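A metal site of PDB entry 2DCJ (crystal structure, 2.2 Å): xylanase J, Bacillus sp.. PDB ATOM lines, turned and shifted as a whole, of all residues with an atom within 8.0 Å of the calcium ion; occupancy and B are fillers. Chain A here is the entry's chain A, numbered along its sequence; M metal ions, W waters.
The side-chain hydroxyl (OG) of Ser 243 lies within hydrogen-bond range of the backbone carbonyl oxygen (O) of Glu 240, 2.8 Å away. The backbone carbonyl oxygen (O) of Asp 349 sits close to the backbone NH (N) of Ala 241 (2.8 Å). NH1 of Arg 286 lies within salt-bridge range of OD2 of Asp 349 (2.9 Å). N of Ile 254 is in hydrogen-bond range of O of Gly 260.
Gly 260 touches the calcium ion (CA to CA, 3.9 Å). Within 4 Å of the calcium ion: Glu 240, Glu 242, Asn 259, Gly 260 and Asp 349. The nearest printed residue that does not touch the calcium ion is Ala 241 (4.1 Å).
The calcium ion is bound by the backbone carbonyl oxygen (O) of Asp 349 (2.5 Å), the side-chain carboxylate (OD1) of Asp 349 (2.5 Å), the backbone carbonyl oxygen (O) of Asn 259 (2.5 Å), the side-chain carboxylate (OE1) of Glu 240 (2.5 Å), the side-chain carboxylate (OE2) of Glu 242 (2.6 Å) and water W1 (2.9 Å). The calcium ion has six donor atoms within binding distance. Slightly farther from the calcium ion lies the side-chain carboxylate (OE1) of Glu 242 (3.1 Å).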
ATOM      1  N   ARG A 238      28.590  38.017  -9.960  1.00  0.00           N
ATOM      2  CA  ARG A 238      28.439  36.762 -10.681  1.00  0.00           C
ATOM      3  C   ARG A 238      27.368  35.960 -10.085  1.00  0.00           C
ATOM      4  O   ARG A 238      27.392  35.725  -8.927  1.00  0.00           O
ATOM      5  CB  ARG A 238      29.741  35.965 -10.658  1.00  0.00           C
ATOM      6  CG  ARG A 238      29.583  34.626 -11.449  1.00  0.00           C
ATOM      7  CD  ARG A 238      30.848  33.815 -11.613  1.00  0.00           C
ATOM      8  NE  ARG A 238      31.812  34.559 -12.396  1.00  0.00           N
ATOM      9  CZ  ARG A 238      33.008  34.053 -12.748  1.00  0.00           C
ATOM     10  NH1 ARG A 238      33.298  32.814 -12.454  1.00  0.00           N
ATOM     11  NH2 ARG A 238      33.879  34.753 -13.436  1.00  0.00           N
ATOM     12  N   VAL A 239      26.398  35.514 -10.869  1.00  0.00           N
ATOM     13  CA  VAL A 239      25.328  34.671 -10.410  1.00  0.00           C
ATOM     14  C   VAL A 239      25.361  33.318 -11.202  1.00  0.00           C
ATOM     15  O   VAL A 239      25.217  33.326 -12.432  1.00  0.00           O
ATOM     16  CB  VAL A 239      23.971  35.353 -10.636  1.00  0.00           C
ATOM     17  CG1 VAL A 239      22.852  34.493 -10.089  1.00  0.00           C
ATOM     18  CG2 VAL A 239      23.936  36.789  -9.994  1.00  0.00           C
ATOM     19  N   GLU A 240      25.486  32.209 -10.480  1.00  0.00           N
ATOM     20  CA  GLU A 240      25.606  30.887 -11.023  1.00  0.00           C
ATOM     21  C   GLU A 240      24.270  30.494 -11.540  1.00  0.00           C
ATOM     22  O   GLU A 240      23.300  30.677 -10.884  1.00  0.00           O
ATOM     23  CB  GLU A 240      26.140  29.881  -9.997  1.00  0.00           C
ATOM     24  CG  GLU A 240      27.550  30.211  -9.515  1.00  0.00           C
ATOM     25  CD  GLU A 240      28.612  30.109 -10.595  1.00  0.00           C
ATOM     26  OE1 GLU A 240      28.489  29.325 -11.515  1.00  0.00           O
ATOM     27  OE2 GLU A 240      29.636  30.799 -10.573  1.00  0.00           O
ATOM     28  N   ALA A 241      24.220  29.959 -12.763  1.00  0.00           N
ATOM     29  CA  ALA A 241      22.927  29.650 -13.368  1.00  0.00           C
ATOM     30  C   ALA A 241      22.175  28.630 -12.538  1.00  0.00           C
ATOM     31  O   ALA A 241      20.919  28.629 -12.493  1.00  0.00           O
ATOM     32  CB  ALA A 241      23.126  29.141 -14.828  1.00  0.00           C
ATOM     33  N   GLU A 242      22.924  27.722 -11.931  1.00  0.00           N
ATOM     34  CA  GLU A 242      22.279  26.666 -11.154  1.00  0.00           C
ATOM     35  C   GLU A 242      21.615  27.152  -9.813  1.00  0.00           C
ATOM     36  O   GLU A 242      20.918  26.373  -9.167  1.00  0.00           O
ATOM     37  CB  GLU A 242      23.239  25.485 -10.908  1.00  0.00           C
ATOM     38  CG  GLU A 242      24.492  25.699 -10.060  1.00  0.00           C
ATOM     39  CD  GLU A 242      25.647  26.285 -10.842  1.00  0.00           C
ATOM     40  OE1 GLU A 242      26.826  26.088 -10.498  1.00  0.00           O
ATOM     41  OE2 GLU A 242      25.362  27.006 -11.836  1.00  0.00           O
ATOM     42  N   SER A 243      21.840  28.421  -9.423  1.00  0.00           N
ATOM     43  CA  SER A 243      21.285  28.961  -8.192  1.00  0.00           C
ATOM     44  C   SER A 243      20.067  29.791  -8.543  1.00  0.00           C
ATOM     45  O   SER A 243      19.368  30.289  -7.665  1.00  0.00           O
ATOM     46  CB  SER A 243      22.333  29.814  -7.547  1.00  0.00           C
ATOM     47  OG  SER A 243      22.378  31.091  -8.230  1.00  0.00           O
ATOM     48  N   MET A 244      19.796  29.960  -9.841  1.00  0.00           N
ATOM     49  CA  MET A 244      18.695  30.748 -10.292  1.00  0.00           C
ATOM     50  C   MET A 244      17.372  30.014 -10.157  1.00  0.00           C
ATOM     51  O   MET A 244      17.334  28.847  -9.970  1.00  0.00           O
ATOM     52  CB  MET A 244      18.905  31.265 -11.711  1.00  0.00           C
ATOM     53  CG  MET A 244      20.195  32.104 -11.900  1.00  0.00           C
ATOM     54  SD  MET A 244      20.439  32.601 -13.638  1.00  0.00           S
ATOM     55  CE  MET A 244      22.151  33.327 -13.531  1.00  0.00           C
ATOM     56  N   ILE A 254      23.144  20.699 -15.084  1.00  0.00           N
ATOM     57  CA  ILE A 254      24.111  19.915 -15.805  1.00  0.00           C
ATOM     58  C   ILE A 254      25.439  20.069 -15.127  1.00  0.00           C
ATOM     59  O   ILE A 254      25.626  21.007 -14.370  1.00  0.00           O
ATOM     60  CB  ILE A 254      24.227  20.372 -17.320  1.00  0.00           C
ATOM     61  CG1 ILE A 254      24.608  21.861 -17.452  1.00  0.00           C
ATOM     62  CG2 ILE A 254      22.947  20.035 -18.053  1.00  0.00           C
ATOM     63  CD1 ILE A 254      25.049  22.313 -18.857  1.00  0.00           C
ATOM     64  N   PHE A 258      30.049  22.380 -17.981  1.00  0.00           N
ATOM     65  CA  PHE A 258      30.385  23.064 -16.738  1.00  0.00           C
ATOM     66  C   PHE A 258      29.252  22.773 -15.848  1.00  0.00           C
ATOM     67  O   PHE A 258      28.239  22.254 -16.307  1.00  0.00           O
ATOM     68  CB  PHE A 258      30.507  24.594 -16.967  1.00  0.00           C
ATOM     69  CG  PHE A 258      29.626  25.120 -18.061  1.00  0.00           C
ATOM     70  CD1 PHE A 258      28.254  25.102 -17.925  1.00  0.00           C
ATOM     71  CD2 PHE A 258      30.171  25.704 -19.184  1.00  0.00           C
ATOM     72  CE1 PHE A 258      27.404  25.571 -18.921  1.00  0.00           C
ATOM     73  CE2 PHE A 258      29.332  26.184 -20.187  1.00  0.00           C
ATOM     74  CZ  PHE A 258      27.935  26.107 -20.045  1.00  0.00           C
ATOM     75  N   ASN A 259      29.353  23.204 -14.597  1.00  0.00           N
ATOM     76  CA  ASN A 259      28.152  23.192 -13.690  1.00  0.00           C
ATOM     77  C   ASN A 259      27.217  24.285 -14.045  1.00  0.00           C
ATOM     78  O   ASN A 259      27.641  25.373 -14.166  1.00  0.00           O
ATOM     79  CB  ASN A 259      28.599  23.354 -12.217  1.00  0.00           C
ATOM     80  CG  ASN A 259      29.391  22.158 -11.728  1.00  0.00           C
ATOM     81  OD1 ASN A 259      29.000  21.002 -11.986  1.00  0.00           O
ATOM     82  ND2 ASN A 259      30.487  22.407 -11.060  1.00  0.00           N
ATOM     83  N   GLY A 260      25.940  24.005 -14.279  1.00  0.00           N
ATOM     84  CA  GLY A 260      25.083  25.026 -14.768  1.00  0.00           C
ATOM     85  C   GLY A 260      23.778  24.419 -15.063  1.00  0.00           C
ATOM     86  O   GLY A 260      23.380  23.490 -14.377  1.00  0.00           O
ATOM     87  N   VAL A 261      23.082  24.979 -16.042  1.00  0.00           N
ATOM     88  CA  VAL A 261      21.775  24.490 -16.407  1.00  0.00           C
ATOM     89  C   VAL A 261      21.735  24.355 -17.945  1.00  0.00           C
ATOM     90  O   VAL A 261      22.529  24.953 -18.669  1.00  0.00           O
ATOM     91  CB  VAL A 261      20.595  25.388 -15.939  1.00  0.00           C
ATOM     92  CG1 VAL A 261      20.638  25.763 -14.385  1.00  0.00           C
ATOM     93  CG2 VAL A 261      20.559  26.647 -16.703  1.00  0.00           C
ATOM     94  N   ARG A 286      28.274  33.239 -19.640  1.00  0.00           N
ATOM     95  CA  ARG A 286      29.154  32.138 -20.035  1.00  0.00           C
ATOM     96  C   ARG A 286      28.273  30.966 -20.306  1.00  0.00           C
ATOM     97  O   ARG A 286      27.476  30.540 -19.445  1.00  0.00           O
ATOM     98  CB  ARG A 286      30.141  31.781 -18.988  1.00  0.00           C
ATOM     99  CG  ARG A 286      31.075  30.607 -19.421  1.00  0.00           C
ATOM    100  CD  ARG A 286      32.374  30.494 -18.538  1.00  0.00           C
ATOM    101  NE  ARG A 286      33.430  29.713 -19.149  1.00  0.00           N
ATOM    102  CZ  ARG A 286      33.639  28.414 -18.923  1.00  0.00           C
ATOM    103  NH1 ARG A 286      32.814  27.729 -18.190  1.00  0.00           N
ATOM    104  NH2 ARG A 286      34.685  27.803 -19.448  1.00  0.00           N
ATOM    105  N   LEU A 348      24.168  26.974 -19.860  1.00  0.00           N
ATOM    106  CA  LEU A 348      24.489  28.257 -19.145  1.00  0.00           C
ATOM    107  C   LEU A 348      25.268  27.963 -17.905  1.00  0.00           C
ATOM    108  O   LEU A 348      24.863  27.153 -17.115  1.00  0.00           O
ATOM    109  CB  LEU A 348      23.235  29.035 -18.823  1.00  0.00           C
ATOM    110  CG  LEU A 348      22.177  29.306 -19.875  1.00  0.00           C
ATOM    111  CD1 LEU A 348      21.192  30.380 -19.388  1.00  0.00           C
ATOM    112  CD2 LEU A 348      22.862  29.821 -21.006  1.00  0.00           C
ATOM    113  N   ASP A 349      26.420  28.596 -17.785  1.00  0.00           N
ATOM    114  CA  ASP A 349      27.244  28.430 -16.628  1.00  0.00           C
ATOM    115  C   ASP A 349      26.906  29.539 -15.574  1.00  0.00           C
ATOM    116  O   ASP A 349      26.388  29.267 -14.478  1.00  0.00           O
ATOM    117  CB  ASP A 349      28.702  28.440 -17.061  1.00  0.00           C
ATOM    118  CG  ASP A 349      29.655  28.309 -15.928  1.00  0.00           C
ATOM    119  OD1 ASP A 349      29.235  28.159 -14.764  1.00  0.00           O
ATOM    120  OD2 ASP A 349      30.868  28.440 -16.091  1.00  0.00           O
ATOM    121  N   TYR A 350      27.176  30.789 -15.900  1.00  0.00           N
ATOM    122  CA  TYR A 350      26.834  31.873 -14.977  1.00  0.00           C
ATOM    123  C   TYR A 350      26.533  33.122 -15.784  1.00  0.00           C
ATOM    124  O   TYR A 350      26.994  33.213 -16.944  1.00  0.00           O
ATOM    125  CB  TYR A 350      28.010  32.130 -14.000  1.00  0.00           C
ATOM    126  CG  TYR A 350      29.302  32.521 -14.660  1.00  0.00           C
ATOM    127  CD1 TYR A 350      29.461  33.772 -15.181  1.00  0.00           C
ATOM    128  CD2 TYR A 350      30.345  31.607 -14.819  1.00  0.00           C
ATOM    129  CE1 TYR A 350      30.614  34.146 -15.805  1.00  0.00           C
ATOM    130  CE2 TYR A 350      31.529  31.982 -15.440  1.00  0.00           C
ATOM    131  CZ  TYR A 350      31.653  33.248 -15.958  1.00  0.00           C
ATOM    132  OH  TYR A 350      32.835  33.661 -16.564  1.00  0.00           O
ATOM    133  N   LEU A 351      25.893  34.105 -15.121  1.00  0.00           N
ATOM    134  CA  LEU A 351      25.731  35.449 -15.641  1.00  0.00           C
ATOM    135  C   LEU A 351      26.456  36.432 -14.740  1.00  0.00           C
ATOM    136  O   LEU A 351      26.335  36.401 -13.533  1.00  0.00           O
ATOM    137  CB  LEU A 351      24.299  35.781 -15.744  1.00  0.00           C
ATOM    138  CG  LEU A 351      24.053  37.201 -16.276  1.00  0.00           C
ATOM    139  CD1 LEU A 351      24.224  37.299 -17.766  1.00  0.00           C
ATOM    140  CD2 LEU A 351      22.553  37.518 -15.949  1.00  0.00           C
HETATM  141 CA    CA M   1      27.536  27.610 -13.076  1.00  0.00          CA
HETATM  142  O   HOH W   1      29.041  26.733 -10.801  1.00  0.00           O
